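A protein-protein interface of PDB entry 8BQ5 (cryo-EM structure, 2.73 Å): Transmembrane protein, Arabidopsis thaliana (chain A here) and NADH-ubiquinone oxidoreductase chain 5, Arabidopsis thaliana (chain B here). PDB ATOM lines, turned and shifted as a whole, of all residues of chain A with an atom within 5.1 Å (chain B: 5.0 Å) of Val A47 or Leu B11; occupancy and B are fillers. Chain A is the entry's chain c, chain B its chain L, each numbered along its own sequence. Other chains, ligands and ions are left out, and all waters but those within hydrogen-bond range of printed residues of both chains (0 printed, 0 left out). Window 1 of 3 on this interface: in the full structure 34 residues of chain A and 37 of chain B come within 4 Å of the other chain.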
ATOM      1  N   GLY A  43     -22.074 -27.532   7.444  1.00  0.00           N
ATOM      2  CA  GLY A  43     -21.567 -28.006   8.722  1.00  0.00           C
ATOM      3  C   GLY A  43     -20.218 -27.411   9.075  1.00  0.00           C
ATOM      4  O   GLY A  43     -20.001 -26.951  10.198  1.00  0.00           O
ATOM      5  N   VAL A  44     -19.293 -27.401   8.113  1.00  0.00           N
ATOM      6  CA  VAL A  44     -17.940 -26.923   8.386  1.00  0.00           C
ATOM      7  C   VAL A  44     -17.949 -25.430   8.689  1.00  0.00           C
ATOM      8  O   VAL A  44     -17.233 -24.958   9.582  1.00  0.00           O
ATOM      9  CB  VAL A  44     -17.009 -27.274   7.213  1.00  0.00           C
ATOM     10  CG1 VAL A  44     -15.791 -26.360   7.186  1.00  0.00           C
ATOM     11  CG2 VAL A  44     -16.584 -28.726   7.331  1.00  0.00           C
ATOM     12  N   PHE A  45     -18.769 -24.667   7.965  1.00  0.00           N
ATOM     13  CA  PHE A  45     -18.932 -23.251   8.280  1.00  0.00           C
ATOM     14  C   PHE A  45     -19.508 -23.065   9.677  1.00  0.00           C
ATOM     15  O   PHE A  45     -19.109 -22.147  10.403  1.00  0.00           O
ATOM     16  CB  PHE A  45     -19.813 -22.578   7.226  1.00  0.00           C
ATOM     17  CG  PHE A  45     -20.407 -21.269   7.667  1.00  0.00           C
ATOM     18  CD1 PHE A  45     -19.642 -20.116   7.685  1.00  0.00           C
ATOM     19  CD2 PHE A  45     -21.742 -21.187   8.033  1.00  0.00           C
ATOM     20  CE1 PHE A  45     -20.190 -18.909   8.081  1.00  0.00           C
ATOM     21  CE2 PHE A  45     -22.295 -19.984   8.430  1.00  0.00           C
ATOM     22  CZ  PHE A  45     -21.518 -18.843   8.453  1.00  0.00           C
ATOM     23  N   LEU A  46     -20.448 -23.927  10.070  1.00  0.00           N
ATOM     24  CA  LEU A  46     -20.976 -23.873  11.429  1.00  0.00           C
ATOM     25  C   LEU A  46     -19.888 -24.151  12.458  1.00  0.00           C
ATOM     26  O   LEU A  46     -19.817 -23.475  13.488  1.00  0.00           O
ATOM     27  CB  LEU A  46     -22.124 -24.868  11.597  1.00  0.00           C
ATOM     28  CG  LEU A  46     -23.480 -24.498  10.993  1.00  0.00           C
ATOM     29  CD1 LEU A  46     -24.547 -25.477  11.457  1.00  0.00           C
ATOM     30  CD2 LEU A  46     -23.867 -23.069  11.333  1.00  0.00           C
ATOM     31  N   VAL A  47     -19.038 -25.150  12.204  1.00  0.00           N
ATOM     32  CA  VAL A  47     -17.939 -25.443  13.123  1.00  0.00           C
ATOM     33  C   VAL A  47     -16.904 -24.327  13.096  1.00  0.00           C
ATOM     34  O   VAL A  47     -16.200 -24.096  14.086  1.00  0.00           O
ATOM     35  CB  VAL A  47     -17.313 -26.812  12.791  1.00  0.00           C
ATOM     36  CG1 VAL A  47     -16.201 -27.148  13.770  1.00  0.00           C
ATOM     37  CG2 VAL A  47     -18.375 -27.894  12.836  1.00  0.00           C
ATOM     38  N   CYS A  48     -16.800 -23.613  11.975  1.00  0.00           N
ATOM     39  CA  CYS A  48     -15.847 -22.514  11.889  1.00  0.00           C
ATOM     40  C   CYS A  48     -16.300 -21.312  12.711  1.00  0.00           C
ATOM     41  O   CYS A  48     -15.499 -20.404  12.966  1.00  0.00           O
ATOM     42  CB  CYS A  48     -15.637 -22.127  10.424  1.00  0.00           C
ATOM     43  SG  CYS A  48     -14.473 -23.192   9.522  1.00  0.00           S
ATOM     44  N   ILE A  49     -17.559 -21.287  13.142  1.00  0.00           N
ATOM     45  CA  ILE A  49     -18.070 -20.180  13.950  1.00  0.00           C
ATOM     46  C   ILE A  49     -17.451 -20.212  15.347  1.00  0.00           C
ATOM     47  O   ILE A  49     -16.765 -19.247  15.711  1.00  0.00           O
ATOM     48  CB  ILE A  49     -19.609 -20.173  14.017  1.00  0.00           C
ATOM     49  CG1 ILE A  49     -20.227 -20.096  12.620  1.00  0.00           C
ATOM     50  CG2 ILE A  49     -20.086 -18.999  14.846  1.00  0.00           C
ATOM     51  CD1 ILE A  49     -21.682 -20.536  12.571  1.00  0.00           C
ATOM     52  N   PRO A  50     -17.638 -21.260  16.169  1.00  0.00           N
ATOM     53  CA  PRO A  50     -17.044 -21.213  17.517  1.00  0.00           C
ATOM     54  C   PRO A  50     -15.534 -21.085  17.500  1.00  0.00           C
ATOM     55  O   PRO A  50     -14.959 -20.511  18.433  1.00  0.00           O
ATOM     56  CB  PRO A  50     -17.486 -22.542  18.152  1.00  0.00           C
ATOM     57  CG  PRO A  50     -18.596 -23.035  17.313  1.00  0.00           C
ATOM     58  CD  PRO A  50     -18.279 -22.567  15.934  1.00  0.00           C
ATOM     59  N   ILE A  51     -14.875 -21.603  16.462  1.00  0.00           N
ATOM     60  CA  ILE A  51     -13.423 -21.490  16.358  1.00  0.00           C
ATOM     61  C   ILE A  51     -13.009 -20.030  16.233  1.00  0.00           C
ATOM     62  O   ILE A  51     -12.016 -19.599  16.832  1.00  0.00           O
ATOM     63  CB  ILE A  51     -12.908 -22.325  15.173  1.00  0.00           C
ATOM     64  CG1 ILE A  51     -13.260 -23.798  15.362  1.00  0.00           C
ATOM     65  CG2 ILE A  51     -11.404 -22.172  15.025  1.00  0.00           C
ATOM     66  CD1 ILE A  51     -12.677 -24.693  14.300  1.00  0.00           C
ATOM     67  N   PHE B   7      -6.622 -24.899  11.499  1.00  0.00           N
ATOM     68  CA  PHE B   7      -7.551 -26.007  11.671  1.00  0.00           C
ATOM     69  C   PHE B   7      -8.484 -26.228  10.487  1.00  0.00           C
ATOM     70  O   PHE B   7      -9.213 -27.224  10.479  1.00  0.00           O
ATOM     71  CB  PHE B   7      -8.385 -25.800  12.941  1.00  0.00           C
ATOM     72  CG  PHE B   7      -7.596 -25.943  14.215  1.00  0.00           C
ATOM     73  CD1 PHE B   7      -7.171 -27.185  14.654  1.00  0.00           C
ATOM     74  CD2 PHE B   7      -7.280 -24.828  14.974  1.00  0.00           C
ATOM     75  CE1 PHE B   7      -6.444 -27.314  15.825  1.00  0.00           C
ATOM     76  CE2 PHE B   7      -6.556 -24.951  16.144  1.00  0.00           C
ATOM     77  CZ  PHE B   7      -6.137 -26.195  16.570  1.00  0.00           C
ATOM     78  N   LEU B   8      -8.491 -25.336   9.496  1.00  0.00           N
ATOM     79  CA  LEU B   8      -9.351 -25.547   8.331  1.00  0.00           C
ATOM     80  C   LEU B   8      -8.974 -26.789   7.535  1.00  0.00           C
ATOM     81  O   LEU B   8      -9.881 -27.566   7.187  1.00  0.00           O
ATOM     82  CB  LEU B   8      -9.349 -24.297   7.447  1.00  0.00           C
ATOM     83  CG  LEU B   8     -10.551 -23.367   7.569  1.00  0.00           C
ATOM     84  CD1 LEU B   8     -10.304 -22.155   6.707  1.00  0.00           C
ATOM     85  CD2 LEU B   8     -11.821 -24.070   7.145  1.00  0.00           C
ATOM     86  N   PRO B   9      -7.703 -27.039   7.195  1.00  0.00           N
ATOM     87  CA  PRO B   9      -7.383 -28.311   6.529  1.00  0.00           C
ATOM     88  C   PRO B   9      -7.728 -29.532   7.364  1.00  0.00           C
ATOM     89  O   PRO B   9      -8.049 -30.581   6.796  1.00  0.00           O
ATOM     90  CB  PRO B   9      -5.874 -28.212   6.268  1.00  0.00           C
ATOM     91  CG  PRO B   9      -5.553 -26.783   6.325  1.00  0.00           C
ATOM     92  CD  PRO B   9      -6.539 -26.133   7.234  1.00  0.00           C
ATOM     93  N   LEU B  10      -7.665 -29.435   8.696  1.00  0.00           N
ATOM     94  CA  LEU B  10      -8.062 -30.567   9.529  1.00  0.00           C
ATOM     95  C   LEU B  10      -9.535 -30.901   9.339  1.00  0.00           C
ATOM     96  O   LEU B  10      -9.900 -32.074   9.200  1.00  0.00           O
ATOM     97  CB  LEU B  10      -7.777 -30.275  11.002  1.00  0.00           C
ATOM     98  CG  LEU B  10      -8.153 -31.392  11.984  1.00  0.00           C
ATOM     99  CD1 LEU B  10      -7.466 -32.706  11.622  1.00  0.00           C
ATOM    100  CD2 LEU B  10      -7.856 -31.001  13.424  1.00  0.00           C
ATOM    101  N   LEU B  11     -10.396 -29.883   9.337  1.00  0.00           N
ATOM    102  CA  LEU B  11     -11.824 -30.113   9.151  1.00  0.00           C
ATOM    103  C   LEU B  11     -12.110 -30.669   7.762  1.00  0.00           C
ATOM    104  O   LEU B  11     -12.926 -31.585   7.601  1.00  0.00           O
ATOM    105  CB  LEU B  11     -12.597 -28.816   9.385  1.00  0.00           C
ATOM    106  CG  LEU B  11     -12.570 -28.246  10.803  1.00  0.00           C
ATOM    107  CD1 LEU B  11     -13.489 -27.043  10.896  1.00  0.00           C
ATOM    108  CD2 LEU B  11     -12.962 -29.306  11.828  1.00  0.00           C
ATOM    109  N   GLY B  12     -11.450 -30.120   6.741  1.00  0.00           N
ATOM    110  CA  GLY B  12     -11.622 -30.642   5.396  1.00  0.00           C
ATOM    111  C   GLY B  12     -11.125 -32.068   5.257  1.00  0.00           C
ATOM    112  O   GLY B  12     -11.764 -32.898   4.606  1.00  0.00           O
ATOM    113  N   SER B  13      -9.975 -32.371   5.865  1.00  0.00           N
ATOM    114  CA  SER B  13      -9.474 -33.741   5.869  1.00  0.00           C
ATOM    115  C   SER B  13     -10.424 -34.669   6.612  1.00  0.00           C
ATOM    116  O   SER B  13     -10.638 -35.815   6.198  1.00  0.00           O
ATOM    117  CB  SER B  13      -8.080 -33.785   6.494  1.00  0.00           C
ATOM    118  OG  SER B  13      -7.837 -35.024   7.136  1.00  0.00           O
ATOM    119  N   SER B  14     -11.000 -34.191   7.717  1.00  0.00           N
ATOM    120  CA  SER B  14     -11.906 -35.017   8.506  1.00  0.00           C
ATOM    121  C   SER B  14     -13.183 -35.339   7.738  1.00  0.00           C
ATOM    122  O   SER B  14     -13.714 -36.449   7.842  1.00  0.00           O
ATOM    123  CB  SER B  14     -12.240 -34.315   9.821  1.00  0.00           C
ATOM    124  OG  SER B  14     -11.070 -34.086  10.586  1.00  0.00           O
ATOM    125  N   VAL B  15     -13.702 -34.372   6.980  1.00  0.00           N
ATOM    126  CA  VAL B  15     -14.961 -34.584   6.273  1.00  0.00           C
ATOM    127  C   VAL B  15     -14.776 -35.567   5.125  1.00  0.00           C
ATOM    128  O   VAL B  15     -15.585 -36.484   4.938  1.00  0.00           O
ATOM    129  CB  VAL B  15     -15.530 -33.236   5.791  1.00  0.00           C
ATOM    130  CG1 VAL B  15     -16.471 -33.438   4.615  1.00  0.00           C
ATOM    131  CG2 VAL B  15     -16.246 -32.532   6.933  1.00  0.00           C
ATOM    132  N   CYS B  35     -11.621 -25.830   1.694  1.00  0.00           N
ATOM    133  CA  CYS B  35     -11.133 -25.564   3.044  1.00  0.00           C
ATOM    134  C   CYS B  35      -9.679 -25.111   3.017  1.00  0.00           C
ATOM    135  O   CYS B  35      -9.300 -24.168   3.719  1.00  0.00           O
ATOM    136  CB  CYS B  35     -11.295 -26.803   3.926  1.00  0.00           C
ATOM    137  SG  CYS B  35     -12.999 -27.373   4.150  1.00  0.00           S
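O of Val A44 sits at hydrogen-bond distance from SG of Cys A48, 3.3 Å away.
Of the 9 printed residues of chain A, 3 touch a printed residue of chain B.
Hydrophobic or aromatic side chains of chain A within 4 Å of the printed part of chain B: Val A44 and Val A47.
Of the 10 printed residues of chain B, 3 touch a printed residue of chain A.
Printed residues of chain B that touch a printed residue of chain A: Leu B8, Leu B11 and Val B15.
Printed residues of chain B within 4 Å of Val A44: Val B15 (3.8 Å).
Val A47 touches just one residue of chain B: Leu B11 (3.95 Å).
Printed residues of chain B within 4 Å of Cys A48: Leu B8 (3.7 Å).
Pro A50 touches none of the printed residues of chain B.
Of the printed residues of chain A, Leu B8 touches Cys A48.
Printed residues of chain A within 4 Å of Val B15: Val A44.
The nearest printed residue of chain B that does not touch Val A47 is Phe B7 (7.7 Å).
The nearest printed residue of chain A that does not touch Val B15 is Gly A43 (6.8 Å).
Val B15 touches Val A44 (CG2 to CG2, 3.8 Å).
Val A47 touches Leu B11.
Leu B8 touches Cys A48.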
